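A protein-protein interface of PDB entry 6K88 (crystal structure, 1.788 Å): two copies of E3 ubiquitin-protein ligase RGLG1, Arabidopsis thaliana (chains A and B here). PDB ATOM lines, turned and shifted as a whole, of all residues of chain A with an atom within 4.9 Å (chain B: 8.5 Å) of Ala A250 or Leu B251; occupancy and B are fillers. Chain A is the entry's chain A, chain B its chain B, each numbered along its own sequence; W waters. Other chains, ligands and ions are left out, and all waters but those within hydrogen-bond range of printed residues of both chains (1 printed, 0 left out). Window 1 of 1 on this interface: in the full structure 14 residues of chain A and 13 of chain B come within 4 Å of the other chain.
Of the printed residues of chain B, Thr A247 touches Phe B82.
Phe A249 touches none of the printed residues of chain B.
Printed residues of chain A within 4 Å of Leu B251: Thr A78, Phe A82 and Ala A250.
Of the printed residues of chain A, Ser B252 touches Phe A82.
Of the printed residues of chain A, Leu B254 touches Leu A251.
Hydrophobic or aromatic side chains of chain A that line the printed part of chain B: Phe A82, Ala A250 and Leu A251.
Hydrophobic or aromatic side chains of chain B within 4 Å of the printed part of chain A: Phe B82, Leu B251, Leu B254 and Met B255.
Among the printed residues, no Asp or Glu carboxylate lies within 4 Å of a Lys or Arg side-chain nitrogen of the other chain.
Water W1 lies within hydrogen-bond range of the backbone carbonyl oxygen (O) of Met B255 (3.0 Å) and the backbone carbonyl oxygen (O) of Leu A254 (3.1 Å).
O of Thr A78 touches CG2 of Thr B247 (3.7 Å).
O of Thr A78 touches CD1 of Leu B251, at 3.6 Å.
Phe A82 touches Glu B248 (CE1 to CG, 3.6 Å).
Leu B251 touches Phe A82.
OG of Ser B252 touches CE1 of Phe A82, at 3.5 Å.
Phe A82 touches Met B255 (CZ to CE, 3.9 Å).
CG2 of Thr A247 touches CZ of Phe B82 (3.3 Å).
Phe B82 touches Glu A248 (CE1 to OE2, 3.3 Å).
Ala A250 touches Leu B251 (CB to CD2, 3.8 Å).
Leu B254 touches Leu A251 (CB to CD1, 3.9 Å).
The backbone carbonyl oxygen of Glu A248 sits at hydrogen-bond distance from the side-chain hydroxyl of Ser A252 (3.1 Å).
The side-chain amide nitrogen (NE2) of Gln B228 is in hydrogen-bond range of the backbone carbonyl oxygen (O) of Ser B252 (2.7 Å).
The backbone carbonyl oxygen (O) of Glu B248 is in hydrogen-bond range of the side-chain hydroxyl (OG) of Ser B252, 3.0 Å away.
Thr A78 touches Thr B247, but with the chains exchanged Thr A247 does not touch Thr B78 (5.0 Å).
Phe A82 touches Leu B251, but with the chains exchanged Leu A251 does not touch Phe B82 (5.0 Å).
Phe A82 touches Ser B252, but with the chains exchanged Ser A252 does not touch Phe B82 (9.6 Å).
Leu A251 touches Leu B254, but with the chains exchanged Leu A254 does not touch Leu B251 (5.0 Å).
Positions printed for both chains: 78, 79, 82, 246, 247, 248, 249, 250, 251, 252, 253 and 254.
Of the 10 pairs that touch across the chains among the printed residues, 2 have their exchanged pair printed and touching as well.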
ATOM      1  N   THR A  78      25.734 -19.453   4.110  1.00  0.00           N
ATOM      2  CA  THR A  78      25.267 -18.828   5.338  1.00  0.00           C
ATOM      3  C   THR A  78      24.046 -19.519   5.918  1.00  0.00           C
ATOM      4  O   THR A  78      24.183 -20.455   6.707  1.00  0.00           O
ATOM      5  CB  THR A  78      24.955 -17.326   5.117  1.00  0.00           C
ATOM      6  OG1 THR A  78      24.036 -17.157   4.020  1.00  0.00           O
ATOM      7  CG2 THR A  78      26.233 -16.582   4.818  1.00  0.00           C
ATOM      8  N   LEU A  79      22.861 -19.057   5.524  1.00  0.00           N
ATOM      9  CA  LEU A  79      21.586 -19.612   5.998  1.00  0.00           C
ATOM     10  C   LEU A  79      21.486 -21.125   5.938  1.00  0.00           C
ATOM     11  O   LEU A  79      20.918 -21.750   6.828  1.00  0.00           O
ATOM     12  CB  LEU A  79      20.414 -19.048   5.185  1.00  0.00           C
ATOM     13  CG  LEU A  79      20.187 -17.549   5.190  1.00  0.00           C
ATOM     14  CD1 LEU A  79      18.842 -17.250   4.515  1.00  0.00           C
ATOM     15  CD2 LEU A  79      20.224 -17.045   6.610  1.00  0.00           C
ATOM     16  N   PHE A  82      22.105 -24.061   8.675  1.00  0.00           N
ATOM     17  CA  PHE A  82      21.139 -24.556   9.668  1.00  0.00           C
ATOM     18  C   PHE A  82      20.333 -25.762   9.209  1.00  0.00           C
ATOM     19  O   PHE A  82      19.719 -26.439  10.036  1.00  0.00           O
ATOM     20  CB  PHE A  82      20.162 -23.449  10.071  1.00  0.00           C
ATOM     21  CG  PHE A  82      20.779 -22.384  10.922  1.00  0.00           C
ATOM     22  CD1 PHE A  82      20.935 -22.580  12.291  1.00  0.00           C
ATOM     23  CD2 PHE A  82      21.214 -21.193  10.358  1.00  0.00           C
ATOM     24  CE1 PHE A  82      21.507 -21.601  13.087  1.00  0.00           C
ATOM     25  CE2 PHE A  82      21.785 -20.208  11.144  1.00  0.00           C
ATOM     26  CZ  PHE A  82      21.932 -20.411  12.516  1.00  0.00           C
ATOM     27  N   GLU A 246      28.451 -10.938   3.822  1.00  0.00           N
ATOM     28  CA  GLU A 246      27.709 -12.195   3.772  1.00  0.00           C
ATOM     29  C   GLU A 246      27.007 -12.457   5.089  1.00  0.00           C
ATOM     30  O   GLU A 246      25.840 -12.861   5.114  1.00  0.00           O
ATOM     31  CB  GLU A 246      28.636 -13.358   3.402  1.00  0.00           C
ATOM     32  CG  GLU A 246      29.105 -13.276   1.945  1.00  0.00           C
ATOM     33  CD  GLU A 246      29.857 -14.514   1.478  1.00  0.00           C
ATOM     34  OE1 GLU A 246      29.755 -15.569   2.142  1.00  0.00           O
ATOM     35  OE2 GLU A 246      30.547 -14.429   0.439  1.00  0.00           O
ATOM     36  N   THR A 247      27.703 -12.192   6.189  1.00  0.00           N
ATOM     37  CA  THR A 247      27.099 -12.361   7.511  1.00  0.00           C
ATOM     38  C   THR A 247      25.970 -11.352   7.743  1.00  0.00           C
ATOM     39  O   THR A 247      24.927 -11.702   8.303  1.00  0.00           O
ATOM     40  CB  THR A 247      28.144 -12.225   8.631  1.00  0.00           C
ATOM     41  OG1 THR A 247      29.187 -13.184   8.421  1.00  0.00           O
ATOM     42  CG2 THR A 247      27.500 -12.478   9.986  1.00  0.00           C
ATOM     43  N   GLU A 248      26.175 -10.114   7.299  1.00  0.00           N
ATOM     44  CA  GLU A 248      25.133  -9.089   7.383  1.00  0.00           C
ATOM     45  C   GLU A 248      23.893  -9.514   6.609  1.00  0.00           C
ATOM     46  O   GLU A 248      22.761  -9.380   7.094  1.00  0.00           O
ATOM     47  CB  GLU A 248      25.633  -7.741   6.844  1.00  0.00           C
ATOM     48  CG  GLU A 248      26.755  -7.085   7.644  1.00  0.00           C
ATOM     49  CD  GLU A 248      26.369  -6.773   9.078  1.00  0.00           C
ATOM     50  OE1 GLU A 248      25.158  -6.612   9.352  1.00  0.00           O
ATOM     51  OE2 GLU A 248      27.286  -6.689   9.928  1.00  0.00           O
ATOM     52  N   PHE A 249      24.104 -10.013   5.398  1.00  0.00           N
ATOM     53  CA  PHE A 249      22.995 -10.592   4.651  1.00  0.00           C
ATOM     54  C   PHE A 249      22.280 -11.677   5.466  1.00  0.00           C
ATOM     55  O   PHE A 249      21.052 -11.682   5.563  1.00  0.00           O
ATOM     56  CB  PHE A 249      23.451 -11.195   3.325  1.00  0.00           C
ATOM     57  CG  PHE A 249      22.455 -12.157   2.756  1.00  0.00           C
ATOM     58  CD1 PHE A 249      21.319 -11.684   2.097  1.00  0.00           C
ATOM     59  CD2 PHE A 249      22.605 -13.524   2.934  1.00  0.00           C
ATOM     60  CE1 PHE A 249      20.369 -12.563   1.595  1.00  0.00           C
ATOM     61  CE2 PHE A 249      21.655 -14.413   2.443  1.00  0.00           C
ATOM     62  CZ  PHE A 249      20.526 -13.934   1.769  1.00  0.00           C
ATOM     63  N   ALA A 250      23.049 -12.603   6.035  1.00  0.00           N
ATOM     64  CA  ALA A 250      22.460 -13.725   6.766  1.00  0.00           C
ATOM     65  C   ALA A 250      21.648 -13.251   7.975  1.00  0.00           C
ATOM     66  O   ALA A 250      20.517 -13.684   8.199  1.00  0.00           O
ATOM     67  CB  ALA A 250      23.554 -14.697   7.205  1.00  0.00           C
ATOM     68  N   LEU A 251      22.241 -12.357   8.754  1.00  0.00           N
ATOM     69  CA  LEU A 251      21.573 -11.807   9.924  1.00  0.00           C
ATOM     70  C   LEU A 251      20.295 -11.048   9.556  1.00  0.00           C
ATOM     71  O   LEU A 251      19.323 -11.100  10.297  1.00  0.00           O
ATOM     72  CB  LEU A 251      22.536 -10.902  10.692  1.00  0.00           C
ATOM     73  CG  LEU A 251      23.728 -11.702  11.226  1.00  0.00           C
ATOM     74  CD1 LEU A 251      24.734 -10.814  11.966  1.00  0.00           C
ATOM     75  CD2 LEU A 251      23.223 -12.840  12.108  1.00  0.00           C
ATOM     76  N   SER A 252      20.289 -10.362   8.414  1.00  0.00           N
ATOM     77  CA  SER A 252      19.074  -9.690   7.948  1.00  0.00           C
ATOM     78  C   SER A 252      18.022 -10.713   7.576  1.00  0.00           C
ATOM     79  O   SER A 252      16.861 -10.567   7.925  1.00  0.00           O
ATOM     80  CB  SER A 252      19.357  -8.783   6.744  1.00  0.00           C
ATOM     81  OG  SER A 252      20.139  -7.669   7.133  1.00  0.00           O
ATOM     82  N   ALA A 253      18.436 -11.758   6.867  1.00  0.00           N
ATOM     83  CA  ALA A 253      17.499 -12.812   6.481  1.00  0.00           C
ATOM     84  C   ALA A 253      16.887 -13.494   7.691  1.00  0.00           C
ATOM     85  O   ALA A 253      15.734 -13.908   7.649  1.00  0.00           O
ATOM     86  CB  ALA A 253      18.190 -13.848   5.592  1.00  0.00           C
ATOM     87  N   LEU A 254      17.651 -13.596   8.777  1.00  0.00           N
ATOM     88  CA  LEU A 254      17.170 -14.294   9.961  1.00  0.00           C
ATOM     89  C   LEU A 254      16.569 -13.365  11.006  1.00  0.00           C
ATOM     90  O   LEU A 254      16.128 -13.820  12.061  1.00  0.00           O
ATOM     91  CB  LEU A 254      18.304 -15.099  10.590  1.00  0.00           C
ATOM     92  CG  LEU A 254      18.741 -16.300   9.759  1.00  0.00           C
ATOM     93  CD1 LEU A 254      19.709 -17.168  10.537  1.00  0.00           C
ATOM     94  CD2 LEU A 254      17.527 -17.112   9.328  1.00  0.00           C
ATOM     95  N   THR B  78      35.463 -16.946  12.187  1.00  0.00           N
ATOM     96  CA  THR B  78      34.103 -16.592  11.791  1.00  0.00           C
ATOM     97  C   THR B  78      33.589 -15.241  12.296  1.00  0.00           C
ATOM     98  O   THR B  78      32.702 -14.665  11.671  1.00  0.00           O
ATOM     99  CB  THR B  78      33.103 -17.676  12.249  1.00  0.00           C
ATOM    100  OG1 THR B  78      33.153 -17.804  13.675  1.00  0.00           O
ATOM    101  CG2 THR B  78      33.438 -19.015  11.612  1.00  0.00           C
ATOM    102  N   LEU B  79      34.123 -14.743  13.412  1.00  0.00           N
ATOM    103  CA  LEU B  79      33.619 -13.501  14.021  1.00  0.00           C
ATOM    104  C   LEU B  79      34.621 -12.343  13.986  1.00  0.00           C
ATOM    105  O   LEU B  79      34.244 -11.191  14.214  1.00  0.00           O
ATOM    106  CB  LEU B  79      33.208 -13.742  15.484  1.00  0.00           C
ATOM    107  CG  LEU B  79      32.106 -14.771  15.753  1.00  0.00           C
ATOM    108  CD1 LEU B  79      31.952 -14.997  17.239  1.00  0.00           C
ATOM    109  CD2 LEU B  79      30.792 -14.316  15.149  1.00  0.00           C
ATOM    110  N   PHE B  82      34.194  -8.837  12.654  1.00  0.00           N
ATOM    111  CA  PHE B  82      33.389  -7.856  13.366  1.00  0.00           C
ATOM    112  C   PHE B  82      34.165  -7.094  14.429  1.00  0.00           C
ATOM    113  O   PHE B  82      33.575  -6.420  15.274  1.00  0.00           O
ATOM    114  CB  PHE B  82      32.171  -8.538  13.976  1.00  0.00           C
ATOM    115  CG  PHE B  82      31.234  -9.067  12.944  1.00  0.00           C
ATOM    116  CD1 PHE B  82      30.219  -8.269  12.446  1.00  0.00           C
ATOM    117  CD2 PHE B  82      31.398 -10.341  12.430  1.00  0.00           C
ATOM    118  CE1 PHE B  82      29.365  -8.739  11.478  1.00  0.00           C
ATOM    119  CE2 PHE B  82      30.550 -10.816  11.459  1.00  0.00           C
ATOM    120  CZ  PHE B  82      29.533 -10.012  10.984  1.00  0.00           C
ATOM    121  N   VAL B 200      27.625 -12.314  24.521  1.00  0.00           N
ATOM    122  CA  VAL B 200      27.452 -13.629  23.901  1.00  0.00           C
ATOM    123  C   VAL B 200      28.173 -14.674  24.741  1.00  0.00           C
ATOM    124  O   VAL B 200      29.399 -14.630  24.879  1.00  0.00           O
ATOM    125  CB  VAL B 200      28.001 -13.677  22.446  1.00  0.00           C
ATOM    126  CG1 VAL B 200      27.835 -15.080  21.844  1.00  0.00           C
ATOM    127  CG2 VAL B 200      27.288 -12.649  21.577  1.00  0.00           C
ATOM    128  N   GLN B 228      23.029 -13.387  24.884  1.00  0.00           N
ATOM    129  CA  GLN B 228      22.739 -14.528  24.023  1.00  0.00           C
ATOM    130  C   GLN B 228      23.540 -15.735  24.478  1.00  0.00           C
ATOM    131  O   GLN B 228      24.717 -15.603  24.781  1.00  0.00           O
ATOM    132  CB  GLN B 228      23.075 -14.208  22.559  1.00  0.00           C
ATOM    133  CG  GLN B 228      23.196 -15.437  21.622  1.00  0.00           C
ATOM    134  CD  GLN B 228      21.859 -16.098  21.329  1.00  0.00           C
ATOM    135  OE1 GLN B 228      20.965 -16.133  22.179  1.00  0.00           O
ATOM    136  NE2 GLN B 228      21.708 -16.613  20.115  1.00  0.00           N
ATOM    137  N   VAL B 230      25.050 -19.445  23.313  1.00  0.00           N
ATOM    138  CA  VAL B 230      25.283 -20.367  22.211  1.00  0.00           C
ATOM    139  C   VAL B 230      25.981 -21.612  22.719  1.00  0.00           C
ATOM    140  O   VAL B 230      27.025 -21.527  23.377  1.00  0.00           O
ATOM    141  CB  VAL B 230      26.142 -19.743  21.108  1.00  0.00           C
ATOM    142  CG1 VAL B 230      26.122 -20.650  19.870  1.00  0.00           C
ATOM    143  CG2 VAL B 230      25.624 -18.401  20.773  1.00  0.00           C
ATOM    144  N   ILE B 235      26.722 -27.663  19.071  1.00  0.00           N
ATOM    145  CA  ILE B 235      26.761 -27.371  17.641  1.00  0.00           C
ATOM    146  C   ILE B 235      27.911 -28.095  16.936  1.00  0.00           C
ATOM    147  O   ILE B 235      27.704 -28.675  15.864  1.00  0.00           O
ATOM    148  CB  ILE B 235      26.862 -25.860  17.373  1.00  0.00           C
ATOM    149  CG1 ILE B 235      25.569 -25.185  17.822  1.00  0.00           C
ATOM    150  CG2 ILE B 235      27.059 -25.593  15.897  1.00  0.00           C
ATOM    151  CD1 ILE B 235      25.620 -23.654  17.776  1.00  0.00           C
ATOM    152  N   ARG B 244      30.111 -25.989   7.793  1.00  0.00           N
ATOM    153  CA  ARG B 244      28.701 -25.672   8.039  1.00  0.00           C
ATOM    154  C   ARG B 244      28.447 -25.536   9.539  1.00  0.00           C
ATOM    155  O   ARG B 244      27.682 -24.672   9.965  1.00  0.00           O
ATOM    156  CB  ARG B 244      27.771 -26.734   7.430  1.00  0.00           C
ATOM    157  CG  ARG B 244      27.819 -26.750   5.891  1.00  0.00           C
ATOM    158  CD  ARG B 244      26.827 -27.733   5.259  1.00  0.00           C
ATOM    159  NE  ARG B 244      25.432 -27.368   5.517  1.00  0.00           N
ATOM    160  CZ  ARG B 244      24.566 -28.154   6.144  1.00  0.00           C
ATOM    161  NH1 ARG B 244      24.938 -29.351   6.571  1.00  0.00           N
ATOM    162  NH2 ARG B 244      23.328 -27.744   6.345  1.00  0.00           N
ATOM    163  N   LYS B 245      29.100 -26.384  10.329  1.00  0.00           N
ATOM    164  CA  LYS B 245      29.017 -26.270  11.783  1.00  0.00           C
ATOM    165  C   LYS B 245      29.591 -24.931  12.233  1.00  0.00           C
ATOM    166  O   LYS B 245      29.004 -24.252  13.081  1.00  0.00           O
ATOM    167  CB  LYS B 245      29.748 -27.438  12.470  1.00  0.00           C
ATOM    168  CG  LYS B 245      29.028 -28.777  12.281  1.00  0.00           C
ATOM    169  CD  LYS B 245      29.590 -29.877  13.174  1.00  0.00           C
ATOM    170  CE  LYS B 245      30.975 -30.294  12.725  1.00  0.00           C
ATOM    171  NZ  LYS B 245      31.458 -31.497  13.468  1.00  0.00           N
ATOM    172  N   GLU B 246      30.728 -24.547  11.666  1.00  0.00           N
ATOM    173  CA  GLU B 246      31.360 -23.284  12.054  1.00  0.00           C
ATOM    174  C   GLU B 246      30.451 -22.101  11.733  1.00  0.00           C
ATOM    175  O   GLU B 246      30.337 -21.159  12.526  1.00  0.00           O
ATOM    176  CB  GLU B 246      32.717 -23.113  11.372  1.00  0.00           C
ATOM    177  CG  GLU B 246      33.788 -24.091  11.881  1.00  0.00           C
ATOM    178  CD  GLU B 246      35.180 -23.795  11.330  1.00  0.00           C
ATOM    179  OE1 GLU B 246      35.399 -22.693  10.780  1.00  0.00           O
ATOM    180  OE2 GLU B 246      36.060 -24.674  11.455  1.00  0.00           O
ATOM    181  N   THR B 247      29.796 -22.147  10.574  1.00  0.00           N
ATOM    182  CA  THR B 247      28.883 -21.069  10.196  1.00  0.00           C
ATOM    183  C   THR B 247      27.645 -21.070  11.058  1.00  0.00           C
ATOM    184  O   THR B 247      27.150 -20.006  11.433  1.00  0.00           O
ATOM    185  CB  THR B 247      28.483 -21.168   8.718  1.00  0.00           C
ATOM    186  OG1 THR B 247      29.668 -21.034   7.934  1.00  0.00           O
ATOM    187  CG2 THR B 247      27.485 -20.059   8.334  1.00  0.00           C
ATOM    188  N   GLU B 248      27.140 -22.250  11.395  1.00  0.00           N
ATOM    189  CA  GLU B 248      25.988 -22.314  12.284  1.00  0.00           C
ATOM    190  C   GLU B 248      26.328 -21.699  13.637  1.00  0.00           C
ATOM    191  O   GLU B 248      25.502 -21.003  14.236  1.00  0.00           O
ATOM    192  CB  GLU B 248      25.508 -23.756  12.485  1.00  0.00           C
ATOM    193  CG  GLU B 248      24.340 -23.859  13.459  1.00  0.00           C
ATOM    194  CD  GLU B 248      23.869 -25.285  13.686  1.00  0.00           C
ATOM    195  OE1 GLU B 248      22.948 -25.476  14.515  1.00  0.00           O
ATOM    196  OE2 GLU B 248      24.411 -26.215  13.042  1.00  0.00           O
ATOM    197  N   PHE B 249      27.538 -21.965  14.124  1.00  0.00           N
ATOM    198  CA  PHE B 249      27.966 -21.366  15.388  1.00  0.00           C
ATOM    199  C   PHE B 249      27.999 -19.827  15.296  1.00  0.00           C
ATOM    200  O   PHE B 249      27.429 -19.124  16.132  1.00  0.00           O
ATOM    201  CB  PHE B 249      29.353 -21.864  15.808  1.00  0.00           C
ATOM    202  CG  PHE B 249      29.994 -20.995  16.860  1.00  0.00           C
ATOM    203  CD1 PHE B 249      29.543 -21.041  18.174  1.00  0.00           C
ATOM    204  CD2 PHE B 249      30.996 -20.094  16.527  1.00  0.00           C
ATOM    205  CE1 PHE B 249      30.102 -20.222  19.149  1.00  0.00           C
ATOM    206  CE2 PHE B 249      31.567 -19.266  17.500  1.00  0.00           C
ATOM    207  CZ  PHE B 249      31.119 -19.334  18.812  1.00  0.00           C
ATOM    208  N   ALA B 250      28.671 -19.318  14.272  1.00  0.00           N
ATOM    209  CA  ALA B 250      28.835 -17.877  14.096  1.00  0.00           C
ATOM    210  C   ALA B 250      27.493 -17.133  14.002  1.00  0.00           C
ATOM    211  O   ALA B 250      27.311 -16.091  14.635  1.00  0.00           O
ATOM    212  CB  ALA B 250      29.675 -17.603  12.875  1.00  0.00           C
ATOM    213  N   LEU B 251      26.547 -17.660  13.225  1.00  0.00           N
ATOM    214  CA  LEU B 251      25.251 -17.004  13.107  1.00  0.00           C
ATOM    215  C   LEU B 251      24.425 -17.125  14.388  1.00  0.00           C
ATOM    216  O   LEU B 251      23.723 -16.193  14.758  1.00  0.00           O
ATOM    217  CB  LEU B 251      24.469 -17.569  11.908  1.00  0.00           C
ATOM    218  CG  LEU B 251      25.238 -17.366  10.603  1.00  0.00           C
ATOM    219  CD1 LEU B 251      24.532 -18.072   9.438  1.00  0.00           C
ATOM    220  CD2 LEU B 251      25.390 -15.870  10.311  1.00  0.00           C
ATOM    221  N   SER B 252      24.515 -18.263  15.073  1.00  0.00           N
ATOM    222  CA  SER B 252      23.809 -18.425  16.333  1.00  0.00           C
ATOM    223  C   SER B 252      24.353 -17.433  17.350  1.00  0.00           C
ATOM    224  O   SER B 252      23.596 -16.877  18.138  1.00  0.00           O
ATOM    225  CB  SER B 252      23.935 -19.860  16.861  1.00  0.00           C
ATOM    226  OG  SER B 252      23.169 -20.756  16.064  1.00  0.00           O
ATOM    227  N   ALA B 253      25.662 -17.201  17.299  1.00  0.00           N
ATOM    228  CA  ALA B 253      26.309 -16.278  18.223  1.00  0.00           C
ATOM    229  C   ALA B 253      25.797 -14.847  18.038  1.00  0.00           C
ATOM    230  O   ALA B 253      25.530 -14.152  19.017  1.00  0.00           O
ATOM    231  CB  ALA B 253      27.834 -16.333  18.054  1.00  0.00           C
ATOM    232  N   LEU B 254      25.641 -14.426  16.779  1.00  0.00           N
ATOM    233  CA  LEU B 254      25.257 -13.048  16.464  1.00  0.00           C
ATOM    234  C   LEU B 254      23.752 -12.853  16.279  1.00  0.00           C
ATOM    235  O   LEU B 254      23.322 -11.779  15.862  1.00  0.00           O
ATOM    236  CB  LEU B 254      25.985 -12.575  15.203  1.00  0.00           C
ATOM    237  CG  LEU B 254      27.514 -12.623  15.267  1.00  0.00           C
ATOM    238  CD1 LEU B 254      28.144 -12.117  13.970  1.00  0.00           C
ATOM    239  CD2 LEU B 254      28.013 -11.813  16.451  1.00  0.00           C
ATOM    240  N   MET B 255      22.965 -13.872  16.623  1.00  0.00           N
ATOM    241  CA  MET B 255      21.523 -13.917  16.345  1.00  0.00           C
ATOM    242  C   MET B 255      20.678 -12.865  17.074  1.00  0.00           C
ATOM    243  O   MET B 255      19.570 -12.529  16.634  1.00  0.00           O
ATOM    244  CB  MET B 255      20.987 -15.312  16.691  1.00  0.00           C
ATOM    245  CG  MET B 255      19.563 -15.591  16.228  1.00  0.00           C
ATOM    246  SD  MET B 255      19.476 -16.259  14.555  1.00  0.00           S
ATOM    247  CE  MET B 255      20.142 -17.899  14.820  1.00  0.00           C
ATOM    248  N   GLU B 256      21.175 -12.349  18.189  1.00  0.00           N
ATOM    249  CA  GLU B 256      20.405 -11.364  18.944  1.00  0.00           C
ATOM    250  C   GLU B 256      20.968  -9.949  18.813  1.00  0.00           C
ATOM    251  O   GLU B 256      20.430  -9.011  19.402  1.00  0.00           O
ATOM    252  CB  GLU B 256      20.324 -11.760  20.422  1.00  0.00           C
ATOM    253  CG  GLU B 256      19.473 -13.008  20.672  1.00  0.00           C
ATOM    254  CD  GLU B 256      19.248 -13.282  22.157  1.00  0.00           C
ATOM    255  OE1 GLU B 256      19.629 -12.432  22.982  1.00  0.00           O
ATOM    256  OE2 GLU B 256      18.676 -14.336  22.497  1.00  0.00           O
ATOM    257  N   ILE B 257      22.044  -9.795  18.047  1.00  0.00           N
ATOM    258  CA  ILE B 257      22.618  -8.474  17.792  1.00  0.00           C
ATOM    259  C   ILE B 257      21.561  -7.594  17.117  1.00  0.00           C
ATOM    260  O   ILE B 257      20.954  -8.010  16.134  1.00  0.00           O
ATOM    261  CB  ILE B 257      23.881  -8.554  16.906  1.00  0.00           C
ATOM    262  CG1 ILE B 257      24.940  -9.444  17.558  1.00  0.00           C
ATOM    263  CG2 ILE B 257      24.459  -7.173  16.645  1.00  0.00           C
ATOM    264  CD1 ILE B 257      25.328  -8.998  18.946  1.00  0.00           C
HETATM  265  O   HOH W   1      17.243 -13.190  14.896  1.00  0.00           O
